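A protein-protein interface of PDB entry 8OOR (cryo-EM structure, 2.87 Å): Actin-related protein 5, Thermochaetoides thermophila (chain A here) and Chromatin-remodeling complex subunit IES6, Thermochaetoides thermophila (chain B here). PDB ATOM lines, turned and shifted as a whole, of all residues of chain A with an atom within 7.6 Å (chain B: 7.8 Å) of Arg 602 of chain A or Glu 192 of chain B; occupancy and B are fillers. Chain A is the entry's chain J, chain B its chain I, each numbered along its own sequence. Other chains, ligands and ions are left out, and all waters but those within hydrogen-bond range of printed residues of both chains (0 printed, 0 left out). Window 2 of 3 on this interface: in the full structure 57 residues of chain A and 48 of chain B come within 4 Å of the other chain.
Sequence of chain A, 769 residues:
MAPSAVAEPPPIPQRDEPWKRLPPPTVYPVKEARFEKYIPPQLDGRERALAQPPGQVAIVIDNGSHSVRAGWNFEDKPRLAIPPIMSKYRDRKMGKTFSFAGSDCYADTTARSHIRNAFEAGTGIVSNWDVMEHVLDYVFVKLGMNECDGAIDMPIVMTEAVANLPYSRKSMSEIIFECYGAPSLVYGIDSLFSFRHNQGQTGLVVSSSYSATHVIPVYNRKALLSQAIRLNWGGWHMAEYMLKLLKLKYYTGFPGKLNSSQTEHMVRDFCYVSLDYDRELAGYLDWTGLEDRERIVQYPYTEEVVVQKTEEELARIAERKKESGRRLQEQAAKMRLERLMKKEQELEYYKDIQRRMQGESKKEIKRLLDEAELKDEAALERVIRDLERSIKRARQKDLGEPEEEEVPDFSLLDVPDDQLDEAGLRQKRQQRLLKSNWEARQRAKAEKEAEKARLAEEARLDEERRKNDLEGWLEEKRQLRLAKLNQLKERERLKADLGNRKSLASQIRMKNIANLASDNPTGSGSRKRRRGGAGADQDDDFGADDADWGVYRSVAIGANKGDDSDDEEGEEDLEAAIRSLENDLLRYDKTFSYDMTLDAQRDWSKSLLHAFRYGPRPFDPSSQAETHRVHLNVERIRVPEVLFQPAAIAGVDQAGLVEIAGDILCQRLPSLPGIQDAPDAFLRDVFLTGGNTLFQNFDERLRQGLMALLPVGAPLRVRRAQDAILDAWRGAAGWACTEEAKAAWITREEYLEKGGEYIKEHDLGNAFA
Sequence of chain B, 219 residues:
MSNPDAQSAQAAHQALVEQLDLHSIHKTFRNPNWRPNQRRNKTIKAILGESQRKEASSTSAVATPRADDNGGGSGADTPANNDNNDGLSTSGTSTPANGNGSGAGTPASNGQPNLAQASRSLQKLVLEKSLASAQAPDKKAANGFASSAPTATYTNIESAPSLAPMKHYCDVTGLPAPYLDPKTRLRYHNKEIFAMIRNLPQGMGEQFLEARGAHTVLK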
ATOM      1  N   GLN A 601      -1.882 -26.693  32.862  1.00  0.00           N
ATOM      2  CA  GLN A 601      -2.971 -25.962  32.226  1.00  0.00           C
ATOM      3  C   GLN A 601      -2.553 -24.528  31.922  1.00  0.00           C
ATOM      4  O   GLN A 601      -3.139 -23.862  31.070  1.00  0.00           O
ATOM      5  CB  GLN A 601      -4.213 -25.976  33.115  1.00  0.00           C
ATOM      6  CG  GLN A 601      -4.040 -25.225  34.423  1.00  0.00           C
ATOM      7  CD  GLN A 601      -5.256 -25.326  35.315  1.00  0.00           C
ATOM      8  OE1 GLN A 601      -6.259 -25.937  34.948  1.00  0.00           O
ATOM      9  NE2 GLN A 601      -5.177 -24.719  36.493  1.00  0.00           N
ATOM     10  N   ARG A 602      -1.532 -24.061  32.635  1.00  0.00           N
ATOM     11  CA  ARG A 602      -0.933 -22.754  32.389  1.00  0.00           C
ATOM     12  C   ARG A 602       0.555 -22.895  32.659  1.00  0.00           C
ATOM     13  O   ARG A 602       0.970 -22.984  33.817  1.00  0.00           O
ATOM     14  CB  ARG A 602      -1.561 -21.687  33.283  1.00  0.00           C
ATOM     15  CG  ARG A 602      -0.818 -20.369  33.330  1.00  0.00           C
ATOM     16  CD  ARG A 602      -0.710 -19.760  31.955  1.00  0.00           C
ATOM     17  NE  ARG A 602       0.123 -18.564  31.955  1.00  0.00           N
ATOM     18  CZ  ARG A 602       0.414 -17.853  30.874  1.00  0.00           C
ATOM     19  NH1 ARG A 602      -0.120 -18.137  29.697  1.00  0.00           N
ATOM     20  NH2 ARG A 602       1.215 -16.796  30.987  1.00  0.00           N
ATOM     21  N   ASP A 603       1.357 -22.895  31.600  1.00  0.00           N
ATOM     22  CA  ASP A 603       2.795 -23.021  31.748  1.00  0.00           C
ATOM     23  C   ASP A 603       3.487 -22.282  30.611  1.00  0.00           C
ATOM     24  O   ASP A 603       2.859 -21.537  29.855  1.00  0.00           O
ATOM     25  CB  ASP A 603       3.194 -24.503  31.829  1.00  0.00           C
ATOM     26  CG  ASP A 603       2.974 -25.263  30.523  1.00  0.00           C
ATOM     27  OD1 ASP A 603       2.883 -24.656  29.440  1.00  0.00           O
ATOM     28  OD2 ASP A 603       2.904 -26.505  30.585  1.00  0.00           O
ATOM     29  N   TRP A 604       4.801 -22.487  30.515  1.00  0.00           N
ATOM     30  CA  TRP A 604       5.612 -21.828  29.501  1.00  0.00           C
ATOM     31  C   TRP A 604       5.103 -22.085  28.092  1.00  0.00           C
ATOM     32  O   TRP A 604       5.228 -21.216  27.226  1.00  0.00           O
ATOM     33  CB  TRP A 604       7.071 -22.257  29.644  1.00  0.00           C
ATOM     34  CG  TRP A 604       7.368 -23.672  29.286  1.00  0.00           C
ATOM     35  CD1 TRP A 604       7.521 -24.711  30.150  1.00  0.00           C
ATOM     36  CD2 TRP A 604       7.607 -24.201  27.979  1.00  0.00           C
ATOM     37  NE1 TRP A 604       7.816 -25.858  29.464  1.00  0.00           N
ATOM     38  CE2 TRP A 604       7.876 -25.571  28.128  1.00  0.00           C
ATOM     39  CE3 TRP A 604       7.608 -23.651  26.697  1.00  0.00           C
ATOM     40  CZ2 TRP A 604       8.142 -26.398  27.049  1.00  0.00           C
ATOM     41  CZ3 TRP A 604       7.870 -24.473  25.628  1.00  0.00           C
ATOM     42  CH2 TRP A 604       8.134 -25.831  25.808  1.00  0.00           C
ATOM     43  N   SER A 605       4.523 -23.249  27.838  1.00  0.00           N
ATOM     44  CA  SER A 605       4.086 -23.551  26.483  1.00  0.00           C
ATOM     45  C   SER A 605       2.850 -22.776  26.053  1.00  0.00           C
ATOM     46  O   SER A 605       2.427 -22.920  24.904  1.00  0.00           O
ATOM     47  CB  SER A 605       3.822 -25.047  26.348  1.00  0.00           C
ATOM     48  OG  SER A 605       3.779 -25.428  24.985  1.00  0.00           O
ATOM     49  N   LYS A 606       2.248 -21.979  26.927  1.00  0.00           N
ATOM     50  CA  LYS A 606       1.222 -21.022  26.540  1.00  0.00           C
ATOM     51  C   LYS A 606       1.653 -19.574  26.719  1.00  0.00           C
ATOM     52  O   LYS A 606       0.820 -18.674  26.593  1.00  0.00           O
ATOM     53  CB  LYS A 606      -0.075 -21.272  27.302  1.00  0.00           C
ATOM     54  CG  LYS A 606      -0.778 -22.554  26.920  1.00  0.00           C
ATOM     55  CD  LYS A 606      -2.131 -22.622  27.588  1.00  0.00           C
ATOM     56  CE  LYS A 606      -2.866 -23.889  27.218  1.00  0.00           C
ATOM     57  NZ  LYS A 606      -4.181 -23.961  27.907  1.00  0.00           N
ATOM     58  N   SER A 607       2.915 -19.327  27.043  1.00  0.00           N
ATOM     59  CA  SER A 607       3.383 -17.979  27.330  1.00  0.00           C
ATOM     60  C   SER A 607       3.909 -17.325  26.061  1.00  0.00           C
ATOM     61  O   SER A 607       4.857 -17.818  25.443  1.00  0.00           O
ATOM     62  CB  SER A 607       4.468 -18.010  28.400  1.00  0.00           C
ATOM     63  OG  SER A 607       4.926 -16.705  28.683  1.00  0.00           O
ATOM     64  N   LEU A 608       3.278 -16.218  25.674  1.00  0.00           N
ATOM     65  CA  LEU A 608       3.771 -15.415  24.566  1.00  0.00           C
ATOM     66  C   LEU A 608       5.173 -14.890  24.827  1.00  0.00           C
ATOM     67  O   LEU A 608       5.989 -14.811  23.907  1.00  0.00           O
ATOM     68  CB  LEU A 608       2.808 -14.260  24.317  1.00  0.00           C
ATOM     69  CG  LEU A 608       3.121 -13.227  23.247  1.00  0.00           C
ATOM     70  CD1 LEU A 608       3.204 -13.857  21.874  1.00  0.00           C
ATOM     71  CD2 LEU A 608       2.042 -12.185  23.285  1.00  0.00           C
ATOM     72  N   LEU A 609       5.479 -14.544  26.076  1.00  0.00           N
ATOM     73  CA  LEU A 609       6.817 -14.074  26.412  1.00  0.00           C
ATOM     74  C   LEU A 609       7.865 -15.172  26.334  1.00  0.00           C
ATOM     75  O   LEU A 609       9.034 -14.884  26.080  1.00  0.00           O
ATOM     76  CB  LEU A 609       6.817 -13.427  27.783  1.00  0.00           C
ATOM     77  CG  LEU A 609       6.079 -12.106  27.768  1.00  0.00           C
ATOM     78  CD1 LEU A 609       5.877 -11.596  29.160  1.00  0.00           C
ATOM     79  CD2 LEU A 609       6.893 -11.126  26.953  1.00  0.00           C
ATOM     80  N   HIS A 610       7.492 -16.421  26.574  1.00  0.00           N
ATOM     81  CA  HIS A 610       8.442 -17.499  26.336  1.00  0.00           C
ATOM     82  C   HIS A 610       8.744 -17.653  24.855  1.00  0.00           C
ATOM     83  O   HIS A 610       9.903 -17.804  24.460  1.00  0.00           O
ATOM     84  CB  HIS A 610       7.911 -18.809  26.907  1.00  0.00           C
ATOM     85  CG  HIS A 610       8.892 -19.930  26.820  1.00  0.00           C
ATOM     86  ND1 HIS A 610       9.776 -20.226  27.833  1.00  0.00           N
ATOM     87  CD2 HIS A 610       9.146 -20.815  25.830  1.00  0.00           C
ATOM     88  CE1 HIS A 610      10.522 -21.253  27.475  1.00  0.00           C
ATOM     89  NE2 HIS A 610      10.159 -21.629  26.264  1.00  0.00           N
ATOM     90  N   ALA A 611       7.709 -17.649  24.023  1.00  0.00           N
ATOM     91  CA  ALA A 611       7.922 -17.696  22.586  1.00  0.00           C
ATOM     92  C   ALA A 611       8.777 -16.527  22.122  1.00  0.00           C
ATOM     93  O   ALA A 611       9.688 -16.697  21.309  1.00  0.00           O
ATOM     94  CB  ALA A 611       6.580 -17.707  21.865  1.00  0.00           C
ATOM     95  N   TYR B 188       0.822  -2.052  24.900  1.00  0.00           N
ATOM     96  CA  TYR B 188       0.949  -3.473  25.164  1.00  0.00           C
ATOM     97  C   TYR B 188      -0.044  -4.269  24.337  1.00  0.00           C
ATOM     98  O   TYR B 188      -1.098  -3.775  23.952  1.00  0.00           O
ATOM     99  CB  TYR B 188       0.830  -3.734  26.675  1.00  0.00           C
ATOM    100  CG  TYR B 188      -0.498  -3.384  27.278  1.00  0.00           C
ATOM    101  CD1 TYR B 188      -1.542  -4.280  27.341  1.00  0.00           C
ATOM    102  CD2 TYR B 188      -0.699  -2.123  27.777  1.00  0.00           C
ATOM    103  CE1 TYR B 188      -2.739  -3.914  27.888  1.00  0.00           C
ATOM    104  CE2 TYR B 188      -1.864  -1.759  28.320  1.00  0.00           C
ATOM    105  CZ  TYR B 188      -2.885  -2.644  28.380  1.00  0.00           C
ATOM    106  OH  TYR B 188      -4.054  -2.230  28.949  1.00  0.00           O
ATOM    107  N   HIS B 189       0.335  -5.506  24.057  1.00  0.00           N
ATOM    108  CA  HIS B 189      -0.411  -6.367  23.158  1.00  0.00           C
ATOM    109  C   HIS B 189      -1.604  -7.038  23.828  1.00  0.00           C
ATOM    110  O   HIS B 189      -2.683  -7.108  23.233  1.00  0.00           O
ATOM    111  CB  HIS B 189       0.549  -7.405  22.593  1.00  0.00           C
ATOM    112  CG  HIS B 189      -0.061  -8.340  21.607  1.00  0.00           C
ATOM    113  ND1 HIS B 189      -0.600  -7.919  20.415  1.00  0.00           N
ATOM    114  CD2 HIS B 189      -0.157  -9.689  21.606  1.00  0.00           C
ATOM    115  CE1 HIS B 189      -1.039  -8.963  19.740  1.00  0.00           C
ATOM    116  NE2 HIS B 189      -0.781 -10.050  20.440  1.00  0.00           N
ATOM    117  N   ASN B 190      -1.448  -7.528  25.054  1.00  0.00           N
ATOM    118  CA  ASN B 190      -2.454  -8.398  25.653  1.00  0.00           C
ATOM    119  C   ASN B 190      -2.290  -8.401  27.167  1.00  0.00           C
ATOM    120  O   ASN B 190      -1.369  -7.794  27.710  1.00  0.00           O
ATOM    121  CB  ASN B 190      -2.409  -9.794  25.039  1.00  0.00           C
ATOM    122  CG  ASN B 190      -1.159 -10.529  25.355  1.00  0.00           C
ATOM    123  OD1 ASN B 190      -0.323 -10.056  26.098  1.00  0.00           O
ATOM    124  ND2 ASN B 190      -0.997 -11.692  24.754  1.00  0.00           N
ATOM    125  N   LYS B 191      -3.221  -9.087  27.838  1.00  0.00           N
ATOM    126  CA  LYS B 191      -3.218  -9.202  29.297  1.00  0.00           C
ATOM    127  C   LYS B 191      -1.948  -9.837  29.851  1.00  0.00           C
ATOM    128  O   LYS B 191      -1.595  -9.583  31.003  1.00  0.00           O
ATOM    129  CB  LYS B 191      -4.455  -9.967  29.758  1.00  0.00           C
ATOM    130  CG  LYS B 191      -4.562 -11.356  29.205  1.00  0.00           C
ATOM    131  CD  LYS B 191      -5.676 -12.135  29.861  1.00  0.00           C
ATOM    132  CE  LYS B 191      -5.184 -12.724  31.161  1.00  0.00           C
ATOM    133  NZ  LYS B 191      -6.231 -13.536  31.842  1.00  0.00           N
ATOM    134  N   GLU B 192      -1.289 -10.712  29.097  1.00  0.00           N
ATOM    135  CA  GLU B 192      -0.024 -11.262  29.572  1.00  0.00           C
ATOM    136  C   GLU B 192       1.043 -10.186  29.712  1.00  0.00           C
ATOM    137  O   GLU B 192       1.794 -10.169  30.691  1.00  0.00           O
ATOM    138  CB  GLU B 192       0.473 -12.341  28.627  1.00  0.00           C
ATOM    139  CG  GLU B 192       1.851 -12.828  28.993  1.00  0.00           C
ATOM    140  CD  GLU B 192       2.178 -14.165  28.384  1.00  0.00           C
ATOM    141  OE1 GLU B 192       1.771 -14.399  27.231  1.00  0.00           O
ATOM    142  OE2 GLU B 192       2.852 -14.980  29.045  1.00  0.00           O
ATOM    143  N   ILE B 193       1.143  -9.301  28.729  1.00  0.00           N
ATOM    144  CA  ILE B 193       2.142  -8.247  28.742  1.00  0.00           C
ATOM    145  C   ILE B 193       1.747  -7.086  29.641  1.00  0.00           C
ATOM    146  O   ILE B 193       2.612  -6.433  30.221  1.00  0.00           O
ATOM    147  CB  ILE B 193       2.401  -7.818  27.290  1.00  0.00           C
ATOM    148  CG1 ILE B 193       3.036  -8.985  26.550  1.00  0.00           C
ATOM    149  CG2 ILE B 193       3.257  -6.592  27.217  1.00  0.00           C
ATOM    150  CD1 ILE B 193       3.406  -8.683  25.173  1.00  0.00           C
ATOM    151  N   PHE B 194       0.460  -6.815  29.798  1.00  0.00           N
ATOM    152  CA  PHE B 194       0.044  -5.861  30.817  1.00  0.00           C
ATOM    153  C   PHE B 194       0.462  -6.328  32.202  1.00  0.00           C
ATOM    154  O   PHE B 194       0.904  -5.528  33.029  1.00  0.00           O
ATOM    155  CB  PHE B 194      -1.461  -5.654  30.764  1.00  0.00           C
ATOM    156  CG  PHE B 194      -1.967  -4.689  31.775  1.00  0.00           C
ATOM    157  CD1 PHE B 194      -1.989  -3.344  31.506  1.00  0.00           C
ATOM    158  CD2 PHE B 194      -2.396  -5.122  33.006  1.00  0.00           C
ATOM    159  CE1 PHE B 194      -2.448  -2.464  32.430  1.00  0.00           C
ATOM    160  CE2 PHE B 194      -2.853  -4.244  33.919  1.00  0.00           C
ATOM    161  CZ  PHE B 194      -2.880  -2.913  33.633  1.00  0.00           C
ATOM    162  N   ALA B 195       0.268  -7.608  32.494  1.00  0.00           N
ATOM    163  CA  ALA B 195       0.677  -8.143  33.782  1.00  0.00           C
ATOM    164  C   ALA B 195       2.170  -7.969  33.999  1.00  0.00           C
ATOM    165  O   ALA B 195       2.602  -7.479  35.045  1.00  0.00           O
ATOM    166  CB  ALA B 195       0.298  -9.619  33.872  1.00  0.00           C
ATOM    167  N   MET B 196       2.971  -8.347  33.003  1.00  0.00           N
ATOM    168  CA  MET B 196       4.416  -8.163  33.068  1.00  0.00           C
ATOM    169  C   MET B 196       4.811  -6.695  33.180  1.00  0.00           C
ATOM    170  O   MET B 196       5.702  -6.347  33.952  1.00  0.00           O
ATOM    171  CB  MET B 196       5.066  -8.806  31.849  1.00  0.00           C
ATOM    172  CG  MET B 196       6.565  -8.819  31.894  1.00  0.00           C
ATOM    173  SD  MET B 196       7.346  -7.322  31.305  1.00  0.00           S
ATOM    174  CE  MET B 196       7.119  -7.581  29.577  1.00  0.00           C
ATOM    175  N   ILE B 197       4.183  -5.830  32.398  1.00  0.00           N
ATOM    176  CA  ILE B 197       4.485  -4.405  32.454  1.00  0.00           C
ATOM    177  C   ILE B 197       4.274  -3.834  33.843  1.00  0.00           C
ATOM    178  O   ILE B 197       5.078  -3.035  34.325  1.00  0.00           O
ATOM    179  CB  ILE B 197       3.644  -3.659  31.411  1.00  0.00           C
ATOM    180  CG1 ILE B 197       4.308  -3.752  30.059  1.00  0.00           C
ATOM    181  CG2 ILE B 197       3.434  -2.233  31.789  1.00  0.00           C
ATOM    182  CD1 ILE B 197       3.422  -3.271  28.979  1.00  0.00           C
ATOM    183  N   ARG B 198       3.178  -4.193  34.494  1.00  0.00           N
ATOM    184  CA  ARG B 198       2.940  -3.705  35.843  1.00  0.00           C
ATOM    185  C   ARG B 198       3.883  -4.291  36.888  1.00  0.00           C
ATOM    186  O   ARG B 198       3.955  -3.754  37.995  1.00  0.00           O
ATOM    187  CB  ARG B 198       1.496  -3.988  36.219  1.00  0.00           C
ATOM    188  CG  ARG B 198       0.521  -3.149  35.458  1.00  0.00           C
ATOM    189  CD  ARG B 198       0.671  -1.724  35.833  1.00  0.00           C
ATOM    190  NE  ARG B 198      -0.311  -0.869  35.191  1.00  0.00           N
ATOM    191  CZ  ARG B 198      -1.440  -0.471  35.757  1.00  0.00           C
ATOM    192  NH1 ARG B 198      -1.781  -0.871  36.966  1.00  0.00           N
ATOM    193  NH2 ARG B 198      -2.238   0.359  35.100  1.00  0.00           N
ATOM    194  N   ASN B 199       4.621  -5.349  36.565  1.00  0.00           N
ATOM    195  CA  ASN B 199       5.582  -5.945  37.482  1.00  0.00           C
ATOM    196  C   ASN B 199       7.029  -5.654  37.101  1.00  0.00           C
ATOM    197  O   ASN B 199       7.932  -6.363  37.549  1.00  0.00           O
ATOM    198  CB  ASN B 199       5.360  -7.453  37.568  1.00  0.00           C
ATOM    199  CG  ASN B 199       3.985  -7.811  38.092  1.00  0.00           C
ATOM    200  OD1 ASN B 199       3.525  -8.938  37.928  1.00  0.00           O
ATOM    201  ND2 ASN B 199       3.315  -6.850  38.712  1.00  0.00           N
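The guanidinium group (NH2) of Arg 602 of chain A is in salt-bridge range of the side-chain carboxylate (OE2) of Glu 192 of chain B, 3.1 Å away.
OE2 of Glu 192 of chain B lies within hydrogen-bond range of OG of Ser 607 of chain A (2.7 Å).
The side-chain carboxylate (OE1) of Glu 192 of chain B sits at hydrogen-bond distance from the backbone NH (N) of Leu 608 of chain A (2.8 Å).
The side-chain hydroxyl (OG) of Ser 607 of chain A is in hydrogen-bond range of the backbone NH (N) of His 610 of chain A (3.3 Å).
The side-chain hydroxyl of Ser 607 of chain A lies close to the backbone NH of Leu 609 of chain A, at 3.4 Å.
The backbone NH of Glu 192 of chain B lies close to the side-chain amide oxygen of Asn 190 of chain B (3.2 Å).
The backbone NH (N) of Ile 193 of chain B lies within hydrogen-bond range of the side-chain amide oxygen (OD1) of Asn 190 of chain B (3.1 Å).
O of Lys 606 of chain A sits at hydrogen-bond distance from NH1 of Arg 602 of chain A (3.3 Å).
Leu 608 of chain A touches His 189 of chain B (CD2 to CD2, 3.7 Å).
Leu 608 of chain A touches Asn 190 of chain B.
N of Leu 609 of chain A touches OE1 of Glu 192 of chain B, at 3.9 Å.
Met 196 of chain B touches Leu 609 of chain A (CG to CD1, 3.96 Å).
Arg 602 of chain A touches one residue of chain B.
Asp 603 of chain A touches none of the printed residues of chain B.
Of the printed residues of chain B, Ser 607 of chain A touches Glu 192 (2.7 Å).
Of the printed residues of chain B, Leu 608 of chain A touches His 189, Asn 190 and Glu 192.
Of the printed residues of chain B, Leu 609 of chain A touches Glu 192 and Met 196.
Of chain A, only Arg 602, Ser 607, Leu 608 and Leu 609 come within 4 Å of Glu 192 of chain B.
Ile 193 of chain B touches none of the printed residues of chain A.
The nearest residue of chain B that does not touch Arg 602 of chain A is Lys 191 of chain B (7.6 Å).
Hydrophobic or aromatic side chains of chain A that line the printed part of chain B: Leu 608 and Leu 609.
Hydrophobic or aromatic side chains of chain B within 4 Å of the printed part of chain A: His 189 and Met 196.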
